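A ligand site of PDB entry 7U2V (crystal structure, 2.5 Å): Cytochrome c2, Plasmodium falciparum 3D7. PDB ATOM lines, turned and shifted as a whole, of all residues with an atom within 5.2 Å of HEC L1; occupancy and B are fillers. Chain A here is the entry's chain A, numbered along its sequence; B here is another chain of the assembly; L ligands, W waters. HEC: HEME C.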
ATOM      1  N   HIS A  37     -25.002 -34.833  21.532  1.00  0.00           N
ATOM      2  CA  HIS A  37     -23.999 -34.707  20.480  1.00  0.00           C
ATOM      3  C   HIS A  37     -23.578 -33.289  20.148  1.00  0.00           C
ATOM      4  O   HIS A  37     -22.546 -33.115  19.496  1.00  0.00           O
ATOM      5  CB  HIS A  37     -24.524 -35.344  19.169  1.00  0.00           C
ATOM      6  CG  HIS A  37     -24.647 -36.839  19.224  1.00  0.00           C
ATOM      7  ND1 HIS A  37     -25.809 -37.501  18.914  1.00  0.00           N
ATOM      8  CD2 HIS A  37     -23.736 -37.792  19.522  1.00  0.00           C
ATOM      9  CE1 HIS A  37     -25.622 -38.802  19.029  1.00  0.00           C
ATOM     10  NE2 HIS A  37     -24.369 -39.008  19.402  1.00  0.00           N
ATOM     11  N   CYS A  38     -24.347 -32.270  20.556  1.00  0.00           N
ATOM     12  CA  CYS A  38     -24.049 -30.917  20.097  1.00  0.00           C
ATOM     13  C   CYS A  38     -23.927 -29.915  21.246  1.00  0.00           C
ATOM     14  O   CYS A  38     -23.196 -28.920  21.121  1.00  0.00           O
ATOM     15  CB  CYS A  38     -25.136 -30.446  19.119  1.00  0.00           C
ATOM     16  SG  CYS A  38     -25.549 -31.627  17.818  1.00  0.00           S
ATOM     17  N   GLN A  40     -22.367 -29.899  23.901  1.00  0.00           N
ATOM     18  CA  GLN A  40     -21.045 -29.738  24.504  1.00  0.00           C
ATOM     19  C   GLN A  40     -20.299 -28.549  23.936  1.00  0.00           C
ATOM     20  O   GLN A  40     -19.472 -27.944  24.640  1.00  0.00           O
ATOM     21  CB  GLN A  40     -20.229 -31.015  24.304  1.00  0.00           C
ATOM     22  CG  GLN A  40     -20.932 -32.279  24.788  1.00  0.00           C
ATOM     23  CD  GLN A  40     -21.612 -33.034  23.664  1.00  0.00           C
ATOM     24  OE1 GLN A  40     -22.589 -32.566  23.079  1.00  0.00           O
ATOM     25  NE2 GLN A  40     -21.097 -34.220  23.358  1.00  0.00           N
ATOM     26  N   CYS A  41     -20.562 -28.182  22.681  1.00  0.00           N
ATOM     27  CA  CYS A  41     -19.914 -27.049  22.041  1.00  0.00           C
ATOM     28  C   CYS A  41     -20.880 -25.963  21.578  1.00  0.00           C
ATOM     29  O   CYS A  41     -20.422 -24.912  21.133  1.00  0.00           O
ATOM     30  CB  CYS A  41     -19.092 -27.498  20.823  1.00  0.00           C
ATOM     31  SG  CYS A  41     -17.958 -28.872  21.099  1.00  0.00           S
ATOM     32  N   HIS A  42     -22.188 -26.192  21.665  1.00  0.00           N
ATOM     33  CA  HIS A  42     -23.167 -25.292  21.075  1.00  0.00           C
ATOM     34  C   HIS A  42     -24.224 -24.918  22.109  1.00  0.00           C
ATOM     35  O   HIS A  42     -24.827 -25.805  22.725  1.00  0.00           O
ATOM     36  CB  HIS A  42     -23.843 -25.930  19.856  1.00  0.00           C
ATOM     37  CG  HIS A  42     -22.966 -25.979  18.647  1.00  0.00           C
ATOM     38  ND1 HIS A  42     -22.657 -24.864  17.902  1.00  0.00           N
ATOM     39  CD2 HIS A  42     -22.333 -27.024  18.052  1.00  0.00           C
ATOM     40  CE1 HIS A  42     -21.871 -25.210  16.893  1.00  0.00           C
ATOM     41  NE2 HIS A  42     -21.658 -26.519  16.966  1.00  0.00           N
ATOM     42  N   TRP A  58     -18.054 -22.643  22.729  1.00  0.00           N
ATOM     43  CA  TRP A  58     -16.995 -22.671  21.727  1.00  0.00           C
ATOM     44  C   TRP A  58     -17.552 -22.340  20.351  1.00  0.00           C
ATOM     45  O   TRP A  58     -17.141 -21.359  19.721  1.00  0.00           O
ATOM     46  CB  TRP A  58     -16.310 -24.034  21.725  1.00  0.00           C
ATOM     47  CG  TRP A  58     -15.212 -24.162  20.707  1.00  0.00           C
ATOM     48  CD1 TRP A  58     -14.539 -23.136  20.106  1.00  0.00           C
ATOM     49  CD2 TRP A  58     -14.665 -25.372  20.169  1.00  0.00           C
ATOM     50  NE1 TRP A  58     -13.611 -23.637  19.218  1.00  0.00           N
ATOM     51  CE2 TRP A  58     -13.665 -25.008  19.248  1.00  0.00           C
ATOM     52  CE3 TRP A  58     -14.928 -26.729  20.380  1.00  0.00           C
ATOM     53  CZ2 TRP A  58     -12.931 -25.956  18.538  1.00  0.00           C
ATOM     54  CZ3 TRP A  58     -14.190 -27.664  19.668  1.00  0.00           C
ATOM     55  CH2 TRP A  58     -13.209 -27.268  18.767  1.00  0.00           C
ATOM     56  N   GLY A  59     -18.487 -23.141  19.867  1.00  0.00           N
ATOM     57  CA  GLY A  59     -19.123 -22.867  18.604  1.00  0.00           C
ATOM     58  C   GLY A  59     -20.201 -21.809  18.739  1.00  0.00           C
ATOM     59  O   GLY A  59     -20.618 -21.421  19.835  1.00  0.00           O
ATOM     60  N   PRO A  60     -20.671 -21.321  17.590  1.00  0.00           N
ATOM     61  CA  PRO A  60     -21.749 -20.321  17.617  1.00  0.00           C
ATOM     62  C   PRO A  60     -23.035 -20.931  18.145  1.00  0.00           C
ATOM     63  O   PRO A  60     -23.241 -22.138  18.124  1.00  0.00           O
ATOM     64  CB  PRO A  60     -21.888 -19.914  16.142  1.00  0.00           C
ATOM     65  CG  PRO A  60     -21.402 -21.106  15.376  1.00  0.00           C
ATOM     66  CD  PRO A  60     -20.300 -21.721  16.218  1.00  0.00           C
ATOM     67  N   LEU A  62     -26.647 -22.192  18.085  1.00  0.00           N
ATOM     68  CA  LEU A  62     -27.479 -22.788  17.052  1.00  0.00           C
ATOM     69  C   LEU A  62     -28.926 -22.328  17.125  1.00  0.00           C
ATOM     70  O   LEU A  62     -29.766 -22.845  16.378  1.00  0.00           O
ATOM     71  CB  LEU A  62     -27.396 -24.316  17.139  1.00  0.00           C
ATOM     72  CG  LEU A  62     -25.991 -24.879  16.880  1.00  0.00           C
ATOM     73  CD1 LEU A  62     -26.007 -26.403  16.933  1.00  0.00           C
ATOM     74  CD2 LEU A  62     -25.445 -24.391  15.547  1.00  0.00           C
ATOM     75  N   VAL A  65     -30.529 -21.034  13.758  1.00  0.00           N
ATOM     76  CA  VAL A  65     -29.592 -21.430  12.712  1.00  0.00           C
ATOM     77  C   VAL A  65     -30.312 -21.856  11.444  1.00  0.00           C
ATOM     78  O   VAL A  65     -29.704 -21.837  10.358  1.00  0.00           O
ATOM     79  CB  VAL A  65     -28.678 -22.569  13.198  1.00  0.00           C
ATOM     80  CG1 VAL A  65     -29.467 -23.871  13.313  1.00  0.00           C
ATOM     81  CG2 VAL A  65     -27.498 -22.748  12.259  1.00  0.00           C
ATOM     82  N   ARG A  68     -30.179 -19.720   8.327  1.00  0.00           N
ATOM     83  CA  ARG A  68     -29.179 -18.697   8.571  1.00  0.00           C
ATOM     84  C   ARG A  68     -28.045 -18.793   7.546  1.00  0.00           C
ATOM     85  O   ARG A  68     -27.773 -19.860   6.985  1.00  0.00           O
ATOM     86  CB  ARG A  68     -28.611 -18.843   9.988  1.00  0.00           C
ATOM     87  CG  ARG A  68     -28.018 -17.569  10.559  1.00  0.00           C
ATOM     88  CD  ARG A  68     -27.904 -17.663  12.078  1.00  0.00           C
ATOM     89  NE  ARG A  68     -26.880 -18.617  12.498  1.00  0.00           N
ATOM     90  CZ  ARG A  68     -26.807 -19.147  13.710  1.00  0.00           C
ATOM     91  NH1 ARG A  68     -27.691 -18.857  14.647  1.00  0.00           N
ATOM     92  NH2 ARG A  68     -25.811 -19.988  13.991  1.00  0.00           N
ATOM     93  N   THR A  69     -27.387 -17.658   7.303  1.00  0.00           N
ATOM     94  CA  THR A  69     -26.223 -17.646   6.428  1.00  0.00           C
ATOM     95  C   THR A  69     -25.038 -18.243   7.191  1.00  0.00           C
ATOM     96  O   THR A  69     -24.645 -17.730   8.243  1.00  0.00           O
ATOM     97  CB  THR A  69     -25.909 -16.222   5.968  1.00  0.00           C
ATOM     98  OG1 THR A  69     -26.991 -15.728   5.168  1.00  0.00           O
ATOM     99  CG2 THR A  69     -24.624 -16.213   5.132  1.00  0.00           C
ATOM    100  N   ALA A  70     -24.474 -19.314   6.652  1.00  0.00           N
ATOM    101  CA  ALA A  70     -23.399 -20.016   7.345  1.00  0.00           C
ATOM    102  C   ALA A  70     -22.161 -19.125   7.473  1.00  0.00           C
ATOM    103  O   ALA A  70     -21.846 -18.341   6.582  1.00  0.00           O
ATOM    104  CB  ALA A  70     -23.033 -21.292   6.600  1.00  0.00           C
ATOM    105  N   GLY A  71     -21.470 -19.258   8.609  1.00  0.00           N
ATOM    106  CA  GLY A  71     -20.261 -18.480   8.815  1.00  0.00           C
ATOM    107  C   GLY A  71     -19.186 -18.761   7.782  1.00  0.00           C
ATOM    108  O   GLY A  71     -18.449 -17.856   7.389  1.00  0.00           O
ATOM    109  N   MET A  72     -19.086 -20.008   7.326  1.00  0.00           N
ATOM    110  CA  MET A  72     -18.075 -20.352   6.330  1.00  0.00           C
ATOM    111  C   MET A  72     -18.303 -19.629   5.010  1.00  0.00           C
ATOM    112  O   MET A  72     -17.436 -19.691   4.131  1.00  0.00           O
ATOM    113  CB  MET A  72     -18.044 -21.855   6.089  1.00  0.00           C
ATOM    114  CG  MET A  72     -19.367 -22.498   5.787  1.00  0.00           C
ATOM    115  SD  MET A  72     -19.144 -24.105   5.005  1.00  0.00           S
ATOM    116  CE  MET A  72     -18.965 -25.162   6.435  1.00  0.00           C
ATOM    117  N   TRP A  92     -28.137 -22.363   5.758  1.00  0.00           N
ATOM    118  CA  TRP A  92     -28.306 -23.588   6.535  1.00  0.00           C
ATOM    119  C   TRP A  92     -29.759 -24.071   6.414  1.00  0.00           C
ATOM    120  O   TRP A  92     -30.572 -23.967   7.335  1.00  0.00           O
ATOM    121  CB  TRP A  92     -27.920 -23.362   7.991  1.00  0.00           C
ATOM    122  CG  TRP A  92     -26.442 -23.412   8.230  1.00  0.00           C
ATOM    123  CD1 TRP A  92     -25.675 -22.462   8.842  1.00  0.00           C
ATOM    124  CD2 TRP A  92     -25.533 -24.464   7.859  1.00  0.00           C
ATOM    125  NE1 TRP A  92     -24.361 -22.849   8.877  1.00  0.00           N
ATOM    126  CE2 TRP A  92     -24.244 -24.076   8.275  1.00  0.00           C
ATOM    127  CE3 TRP A  92     -25.693 -25.695   7.212  1.00  0.00           C
ATOM    128  CZ2 TRP A  92     -23.127 -24.879   8.073  1.00  0.00           C
ATOM    129  CZ3 TRP A  92     -24.578 -26.490   7.015  1.00  0.00           C
ATOM    130  CH2 TRP A  92     -23.314 -26.076   7.440  1.00  0.00           C
ATOM    131  N   LEU A  97     -27.930 -28.688   6.292  1.00  0.00           N
ATOM    132  CA  LEU A  97     -27.746 -29.151   7.667  1.00  0.00           C
ATOM    133  C   LEU A  97     -27.521 -30.651   7.718  1.00  0.00           C
ATOM    134  O   LEU A  97     -26.637 -31.140   8.430  1.00  0.00           O
ATOM    135  CB  LEU A  97     -28.947 -28.752   8.525  1.00  0.00           C
ATOM    136  CG  LEU A  97     -29.027 -27.283   8.951  1.00  0.00           C
ATOM    137  CD1 LEU A  97     -30.360 -26.973   9.615  1.00  0.00           C
ATOM    138  CD2 LEU A  97     -27.878 -26.928   9.879  1.00  0.00           C
ATOM    139  N   TYR A 100     -23.973 -31.436   6.293  1.00  0.00           N
ATOM    140  CA  TYR A 100     -22.921 -31.026   7.219  1.00  0.00           C
ATOM    141  C   TYR A 100     -22.865 -31.970   8.416  1.00  0.00           C
ATOM    142  O   TYR A 100     -21.779 -32.427   8.811  1.00  0.00           O
ATOM    143  CB  TYR A 100     -23.170 -29.598   7.680  1.00  0.00           C
ATOM    144  CG  TYR A 100     -22.200 -29.115   8.729  1.00  0.00           C
ATOM    145  CD1 TYR A 100     -20.953 -28.625   8.381  1.00  0.00           C
ATOM    146  CD2 TYR A 100     -22.544 -29.139  10.073  1.00  0.00           C
ATOM    147  CE1 TYR A 100     -20.068 -28.198   9.338  1.00  0.00           C
ATOM    148  CE2 TYR A 100     -21.665 -28.707  11.042  1.00  0.00           C
ATOM    149  CZ  TYR A 100     -20.417 -28.237  10.668  1.00  0.00           C
ATOM    150  OH  TYR A 100     -19.535 -27.795  11.618  1.00  0.00           O
ATOM    151  N   MET A 101     -24.014 -32.281   9.016  1.00  0.00           N
ATOM    152  CA  MET A 101     -24.033 -33.216  10.128  1.00  0.00           C
ATOM    153  C   MET A 101     -23.474 -34.571   9.724  1.00  0.00           C
ATOM    154  O   MET A 101     -22.846 -35.247  10.553  1.00  0.00           O
ATOM    155  CB  MET A 101     -25.456 -33.370  10.656  1.00  0.00           C
ATOM    156  CG  MET A 101     -25.751 -32.528  11.894  1.00  0.00           C
ATOM    157  SD  MET A 101     -27.480 -32.564  12.417  1.00  0.00           S
ATOM    158  CE  MET A 101     -28.331 -32.158  10.901  1.00  0.00           C
ATOM    159  N   TRP B  58     -14.032 -16.083   8.263  1.00  0.00           N
ATOM    160  CA  TRP B  58     -14.737 -17.216   8.843  1.00  0.00           C
ATOM    161  C   TRP B  58     -14.220 -17.513  10.251  1.00  0.00           C
ATOM    162  O   TRP B  58     -14.965 -17.437  11.225  1.00  0.00           O
ATOM    163  CB  TRP B  58     -14.589 -18.446   7.947  1.00  0.00           C
ATOM    164  CG  TRP B  58     -15.256 -19.680   8.493  1.00  0.00           C
ATOM    165  CD1 TRP B  58     -16.226 -19.720   9.454  1.00  0.00           C
ATOM    166  CD2 TRP B  58     -15.020 -21.036   8.110  1.00  0.00           C
ATOM    167  NE1 TRP B  58     -16.599 -21.019   9.699  1.00  0.00           N
ATOM    168  CE2 TRP B  58     -15.868 -21.848   8.888  1.00  0.00           C
ATOM    169  CE3 TRP B  58     -14.162 -21.641   7.184  1.00  0.00           C
ATOM    170  CZ2 TRP B  58     -15.891 -23.236   8.760  1.00  0.00           C
ATOM    171  CZ3 TRP B  58     -14.192 -23.024   7.068  1.00  0.00           C
ATOM    172  CH2 TRP B  58     -15.052 -23.808   7.854  1.00  0.00           C
ATOM    173  N   VAL B 108      -8.055 -31.135  19.227  1.00  0.00           N
ATOM    174  CA  VAL B 108      -9.352 -30.885  19.840  1.00  0.00           C
ATOM    175  C   VAL B 108      -9.789 -32.085  20.671  1.00  0.00           C
ATOM    176  O   VAL B 108     -10.187 -31.948  21.841  1.00  0.00           O
ATOM    177  CB  VAL B 108     -10.398 -30.528  18.767  1.00  0.00           C
ATOM    178  CG1 VAL B 108     -11.803 -30.555  19.361  1.00  0.00           C
ATOM    179  CG2 VAL B 108     -10.084 -29.177  18.160  1.00  0.00           C
ATOM    180  N   MET B 114     -13.608 -34.733  23.461  1.00  0.00           N
ATOM    181  CA  MET B 114     -14.486 -35.211  22.406  1.00  0.00           C
ATOM    182  C   MET B 114     -14.219 -34.403  21.145  1.00  0.00           C
ATOM    183  O   MET B 114     -13.372 -33.516  21.105  1.00  0.00           O
ATOM    184  CB  MET B 114     -15.960 -35.117  22.833  1.00  0.00           C
ATOM    185  CG  MET B 114     -16.490 -33.693  22.914  1.00  0.00           C
ATOM    186  SD  MET B 114     -18.306 -33.587  22.893  1.00  0.00           S
ATOM    187  CE  MET B 114     -18.725 -34.607  21.472  1.00  0.00           C
ATOM    188  N   ASN B 115     -14.988 -34.717  20.109  1.00  0.00           N
ATOM    189  CA  ASN B 115     -14.958 -33.996  18.843  1.00  0.00           C
ATOM    190  C   ASN B 115     -16.135 -34.498  18.016  1.00  0.00           C
ATOM    191  O   ASN B 115     -16.627 -35.603  18.226  1.00  0.00           O
ATOM    192  CB  ASN B 115     -13.640 -34.196  18.091  1.00  0.00           C
ATOM    193  CG  ASN B 115     -13.539 -33.334  16.856  1.00  0.00           C
ATOM    194  OD1 ASN B 115     -14.018 -32.198  16.828  1.00  0.00           O
ATOM    195  ND2 ASN B 115     -12.923 -33.873  15.801  1.00  0.00           N
ATOM    196  N   PHE B 116     -16.579 -33.662  17.078  1.00  0.00           N
ATOM    197  CA  PHE B 116     -17.695 -34.009  16.211  1.00  0.00           C
ATOM    198  C   PHE B 116     -17.152 -34.333  14.827  1.00  0.00           C
ATOM    199  O   PHE B 116     -16.688 -33.447  14.110  1.00  0.00           O
ATOM    200  CB  PHE B 116     -18.708 -32.867  16.135  1.00  0.00           C
ATOM    201  CG  PHE B 116     -19.883 -33.174  15.259  1.00  0.00           C
ATOM    202  CD1 PHE B 116     -20.677 -34.278  15.494  1.00  0.00           C
ATOM    203  CD2 PHE B 116     -20.185 -32.358  14.181  1.00  0.00           C
ATOM    204  CE1 PHE B 116     -21.755 -34.568  14.679  1.00  0.00           C
ATOM    205  CE2 PHE B 116     -21.259 -32.635  13.364  1.00  0.00           C
ATOM    206  CZ  PHE B 116     -22.050 -33.746  13.611  1.00  0.00           C
ATOM    207  N   LEU B 119     -22.590 -37.508  12.054  1.00  0.00           N
ATOM    208  CA  LEU B 119     -23.577 -38.512  12.438  1.00  0.00           C
ATOM    209  C   LEU B 119     -24.013 -39.245  11.184  1.00  0.00           C
ATOM    210  O   LEU B 119     -24.505 -38.623  10.231  1.00  0.00           O
ATOM    211  CB  LEU B 119     -24.789 -37.877  13.118  1.00  0.00           C
ATOM    212  CG  LEU B 119     -24.720 -37.530  14.605  1.00  0.00           C
ATOM    213  CD1 LEU B 119     -26.130 -37.202  15.101  1.00  0.00           C
ATOM    214  CD2 LEU B 119     -24.119 -38.637  15.429  1.00  0.00           C
ATOM    215  N   ILE B 128     -32.661 -34.113  14.499  1.00  0.00           N
ATOM    216  CA  ILE B 128     -31.944 -32.928  14.971  1.00  0.00           C
ATOM    217  C   ILE B 128     -32.392 -31.690  14.197  1.00  0.00           C
ATOM    218  O   ILE B 128     -32.568 -30.621  14.781  1.00  0.00           O
ATOM    219  CB  ILE B 128     -30.425 -33.138  14.870  1.00  0.00           C
ATOM    220  CG1 ILE B 128     -29.950 -34.090  15.976  1.00  0.00           C
ATOM    221  CG2 ILE B 128     -29.697 -31.795  14.946  1.00  0.00           C
ATOM    222  CD1 ILE B 128     -28.471 -34.384  15.962  1.00  0.00           C
ATOM    223  N   LEU B 132     -33.984 -28.262  15.555  1.00  0.00           N
ATOM    224  CA  LEU B 132     -33.389 -26.958  15.295  1.00  0.00           C
ATOM    225  C   LEU B 132     -34.406 -25.999  14.669  1.00  0.00           C
ATOM    226  O   LEU B 132     -34.301 -24.779  14.858  1.00  0.00           O
ATOM    227  CB  LEU B 132     -32.170 -27.100  14.383  1.00  0.00           C
ATOM    228  CG  LEU B 132     -30.978 -27.870  14.956  1.00  0.00           C
ATOM    229  CD1 LEU B 132     -29.908 -28.066  13.886  1.00  0.00           C
ATOM    230  CD2 LEU B 132     -30.402 -27.169  16.177  1.00  0.00           C
HETATM  231 FE   HEC L   1     -20.847 -27.610  15.494  1.00  0.00          FE
HETATM  232  CHA HEC L   1     -20.059 -24.809  13.669  1.00  0.00           C
HETATM  233  CHB HEC L   1     -23.947 -27.686  14.080  1.00  0.00           C
HETATM  234  CHC HEC L   1     -21.559 -30.526  17.211  1.00  0.00           C
HETATM  235  CHD HEC L   1     -17.976 -27.259  17.325  1.00  0.00           C
HETATM  236  NA  HEC L   1     -21.819 -26.451  14.135  1.00  0.00           N
HETATM  237  C1A HEC L   1     -21.312 -25.350  13.474  1.00  0.00           C
HETATM  238  C2A HEC L   1     -22.322 -24.881  12.545  1.00  0.00           C
HETATM  239  C3A HEC L   1     -23.389 -25.671  12.665  1.00  0.00           C
HETATM  240  C4A HEC L   1     -23.101 -26.677  13.669  1.00  0.00           C
HETATM  241  CMA HEC L   1     -24.702 -25.552  11.871  1.00  0.00           C
HETATM  242  CAA HEC L   1     -22.186 -23.675  11.598  1.00  0.00           C
HETATM  243  CBA HEC L   1     -22.821 -22.462  12.283  1.00  0.00           C
HETATM  244  CGA HEC L   1     -22.868 -21.285  11.341  1.00  0.00           C
HETATM  245  O1A HEC L   1     -23.511 -20.272  11.706  1.00  0.00           O
HETATM  246  O2A HEC L   1     -22.279 -21.370  10.232  1.00  0.00           O
HETATM  247  NB  HEC L   1     -22.459 -28.859  15.654  1.00  0.00           N
HETATM  248  C1B HEC L   1     -23.625 -28.726  14.918  1.00  0.00           C
HETATM  249  C2B HEC L   1     -24.450 -29.883  15.181  1.00  0.00           C
HETATM  250  C3B HEC L   1     -23.804 -30.671  16.056  1.00  0.00           C
HETATM  251  C4B HEC L   1     -22.534 -30.046  16.359  1.00  0.00           C
HETATM  252  CMB HEC L   1     -25.844 -30.094  14.544  1.00  0.00           C
HETATM  253  CAB HEC L   1     -24.256 -32.035  16.627  1.00  0.00           C
HETATM  254  CBB HEC L   1     -25.117 -32.817  15.971  1.00  0.00           C
HETATM  255  NC  HEC L   1     -19.940 -28.699  16.987  1.00  0.00           N
HETATM  256  C1C HEC L   1     -20.399 -29.871  17.557  1.00  0.00           C
HETATM  257  C2C HEC L   1     -19.450 -30.281  18.575  1.00  0.00           C
HETATM  258  C3C HEC L   1     -18.464 -29.367  18.609  1.00  0.00           C
HETATM  259  C4C HEC L   1     -18.752 -28.361  17.605  1.00  0.00           C
HETATM  260  CMC HEC L   1     -19.603 -31.538  19.460  1.00  0.00           C
HETATM  261  CAC HEC L   1     -17.215 -29.352  19.522  1.00  0.00           C
HETATM  262  CBC HEC L   1     -16.726 -30.486  20.035  1.00  0.00           C
HETATM  263  ND  HEC L   1     -19.285 -26.298  15.463  1.00  0.00           N
HETATM  264  C1D HEC L   1     -18.245 -26.288  16.372  1.00  0.00           C
HETATM  265  C2D HEC L   1     -17.482 -25.086  16.158  1.00  0.00           C
HETATM  266  C3D HEC L   1     -18.047 -24.411  15.149  1.00  0.00           C
HETATM  267  C4D HEC L   1     -19.191 -25.166  14.695  1.00  0.00           C
HETATM  268  CMD HEC L   1     -16.222 -24.666  16.946  1.00  0.00           C
HETATM  269  CAD HEC L   1     -17.549 -23.063  14.578  1.00  0.00           C
HETATM  270  CBD HEC L   1     -16.379 -23.336  13.643  1.00  0.00           C
HETATM  271  CGD HEC L   1     -16.858 -24.119  12.452  1.00  0.00           C
HETATM  272  O1D HEC L   1     -17.892 -23.704  11.844  1.00  0.00           O
HETATM  273  O2D HEC L   1     -16.211 -25.144  12.112  1.00  0.00           O
HETATM  274 FE   HEC L   2      -7.860 -21.997  11.652  1.00  0.00          FE
HETATM  275  CHA HEC L   2      -9.600 -21.786  14.585  1.00  0.00           C
HETATM  276  CHB HEC L   2      -4.938 -21.275  13.326  1.00  0.00           C
HETATM  277  CHC HEC L   2      -6.061 -22.593   8.800  1.00  0.00           C
HETATM  278  CHD HEC L   2     -10.790 -22.261   9.899  1.00  0.00           C
HETATM  279  NA  HEC L   2      -7.363 -21.613  13.603  1.00  0.00           N
HETATM  280  C1A HEC L   2      -8.242 -21.553  14.658  1.00  0.00           C
HETATM  281  C2A HEC L   2      -7.485 -21.206  15.848  1.00  0.00           C
HETATM  282  C3A HEC L   2      -6.200 -21.071  15.496  1.00  0.00           C
HETATM  283  C4A HEC L   2      -6.094 -21.322  14.071  1.00  0.00           C
HETATM  284  CMA HEC L   2      -5.031 -20.697  16.438  1.00  0.00           C
HETATM  285  CAA HEC L   2      -8.062 -21.030  17.270  1.00  0.00           C
HETATM  286  CBA HEC L   2      -8.157 -19.538  17.581  1.00  0.00           C
HETATM  287  CGA HEC L   2      -8.736 -19.331  18.963  1.00  0.00           C
HETATM  288  O1A HEC L   2      -8.946 -18.152  19.344  1.00  0.00           O
HETATM  289  O2A HEC L   2      -8.983 -20.339  19.668  1.00  0.00           O
HETATM  290  NB  HEC L   2      -5.867 -21.934  11.148  1.00  0.00           N
HETATM  291  C1B HEC L   2      -4.823 -21.633  11.998  1.00  0.00           C
HETATM  292  C2B HEC L   2      -3.587 -21.743  11.250  1.00  0.00           C
HETATM  293  C3B HEC L   2      -3.897 -22.081   9.988  1.00  0.00           C
HETATM  294  C4B HEC L   2      -5.336 -22.234   9.914  1.00  0.00           C
HETATM  295  CMB HEC L   2      -2.183 -21.464  11.822  1.00  0.00           C
HETATM  296  CAB HEC L   2      -2.939 -22.358   8.804  1.00  0.00           C
HETATM  297  CBB HEC L   2      -1.722 -22.870   9.012  1.00  0.00           C
HETATM  298  NC  HEC L   2      -8.337 -22.400   9.720  1.00  0.00           N
HETATM  299  C1C HEC L   2      -7.441 -22.538   8.688  1.00  0.00           C
HETATM  300  C2C HEC L   2      -8.181 -22.619   7.448  1.00  0.00           C
HETATM  301  C3C HEC L   2      -9.487 -22.523   7.741  1.00  0.00           C
HETATM  302  C4C HEC L   2      -9.613 -22.392   9.176  1.00  0.00           C
HETATM  303  CMC HEC L   2      -7.525 -22.778   6.060  1.00  0.00           C
HETATM  304  CAC HEC L   2     -10.694 -22.565   6.760  1.00  0.00           C
HETATM  305  CBC HEC L   2     -10.607 -23.196   5.584  1.00  0.00           C
HETATM  306  ND  HEC L   2      -9.830 -22.069  12.156  1.00  0.00           N
HETATM  307  C1D HEC L   2     -10.882 -22.079  11.265  1.00  0.00           C
HETATM  308  C2D HEC L   2     -12.101 -21.867  12.020  1.00  0.00           C
HETATM  309  C3D HEC L   2     -11.778 -21.734  13.307  1.00  0.00           C
HETATM  310  C4D HEC L   2     -10.333 -21.862  13.427  1.00  0.00           C
HETATM  311  CMD HEC L   2     -13.521 -21.802  11.434  1.00  0.00           C
HETATM  312  CAD HEC L   2     -12.755 -21.484  14.474  1.00  0.00           C
HETATM  313  CBD HEC L   2     -13.284 -22.829  14.964  1.00  0.00           C
HETATM  314  CGD HEC L   2     -12.194 -23.613  15.646  1.00  0.00           C
HETATM  315  O1D HEC L   2     -11.569 -23.075  16.603  1.00  0.00           O
HETATM  316  O2D HEC L   2     -11.967 -24.779  15.244  1.00  0.00           O
HETATM  317  O   HOH W   1     -20.025 -28.825  14.112  1.00  0.00           O
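CAB of HEC L1 is bonded to SG of Cys 38 (1.8 Å).
The side-chain sulfur of Cys 41 is bonded to a carbon (CAC) of HEC L1, at 1.8 Å.
A ring nitrogen (NE2) of His 42 is bound to an iron atom (FE) of HEC L1 (2.0 Å).
The backbone NH (N) of Gly 71 lies within hydrogen-bond range of an oxygen (O2A) of HEC L1, at 2.8 Å.
An oxygen (O2A) of HEC L1 is in hydrogen-bond range of the indole nitrogen of Trp 92, 2.9 Å away.
O1A of HEC L1 is in salt-bridge range of NH2 of Arg 68.
An oxygen (O1D) of HEC L2 lies within hydrogen-bond range of the indole nitrogen (NE1) of Trp 58 of chain A, 3.4 Å away.
The side-chain amide oxygen (OE1) of Gln 40 lies within hydrogen-bond range of the backbone NH (N) of Cys 38.
The backbone NH (N) of Gly 59 sits at hydrogen-bond distance from the backbone carbonyl oxygen (O) of Cys 41, at 2.9 Å.
O of Pro 60 lies within hydrogen-bond range of ND1 of His 42 (2.8 Å).
The backbone NH of Trp 92 lies within hydrogen-bond range of the backbone carbonyl oxygen of Arg 68.
N of Leu 119 of chain B sits at hydrogen-bond distance from O of Met 101, 2.7 Å away.
The side-chain sulfur (SD) of Met 114 of chain B sits at hydrogen-bond distance from the side-chain amide nitrogen (NE2) of Gln 40.
Merely in contact with HEC L1: His 37 (3.3 Å), Trp 58 of chain A (3.5 Å), Gly 59 (3.7 Å), Pro 60 (3.5 Å), Leu 62 (3.7 Å), Val 65 (3.98 Å), Ala 70 (3.4 Å), Leu 97 (3.99 Å), Tyr 100 (3.5 Å), Met 101 (3.6 Å), Trp 58 of chain B (3.7 Å), Met 114 of chain B (3.8 Å), Phe 116 of chain B (3.6 Å) and Ile 128 of chain B (3.7 Å).
Hydrophobic or aromatic side chains within 4 Å of HEC L1: His 42, Trp 58 of chain A, Pro 60, Leu 62, Val 65, Ala 70, Trp 92, Leu 97, Tyr 100, Met 101, Trp 58 of chain B, Met 114 of chain B, Phe 116 of chain B and Ile 128 of chain B.
Of the 27 residues printed, 20 come within 4 Å of HEC L1.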
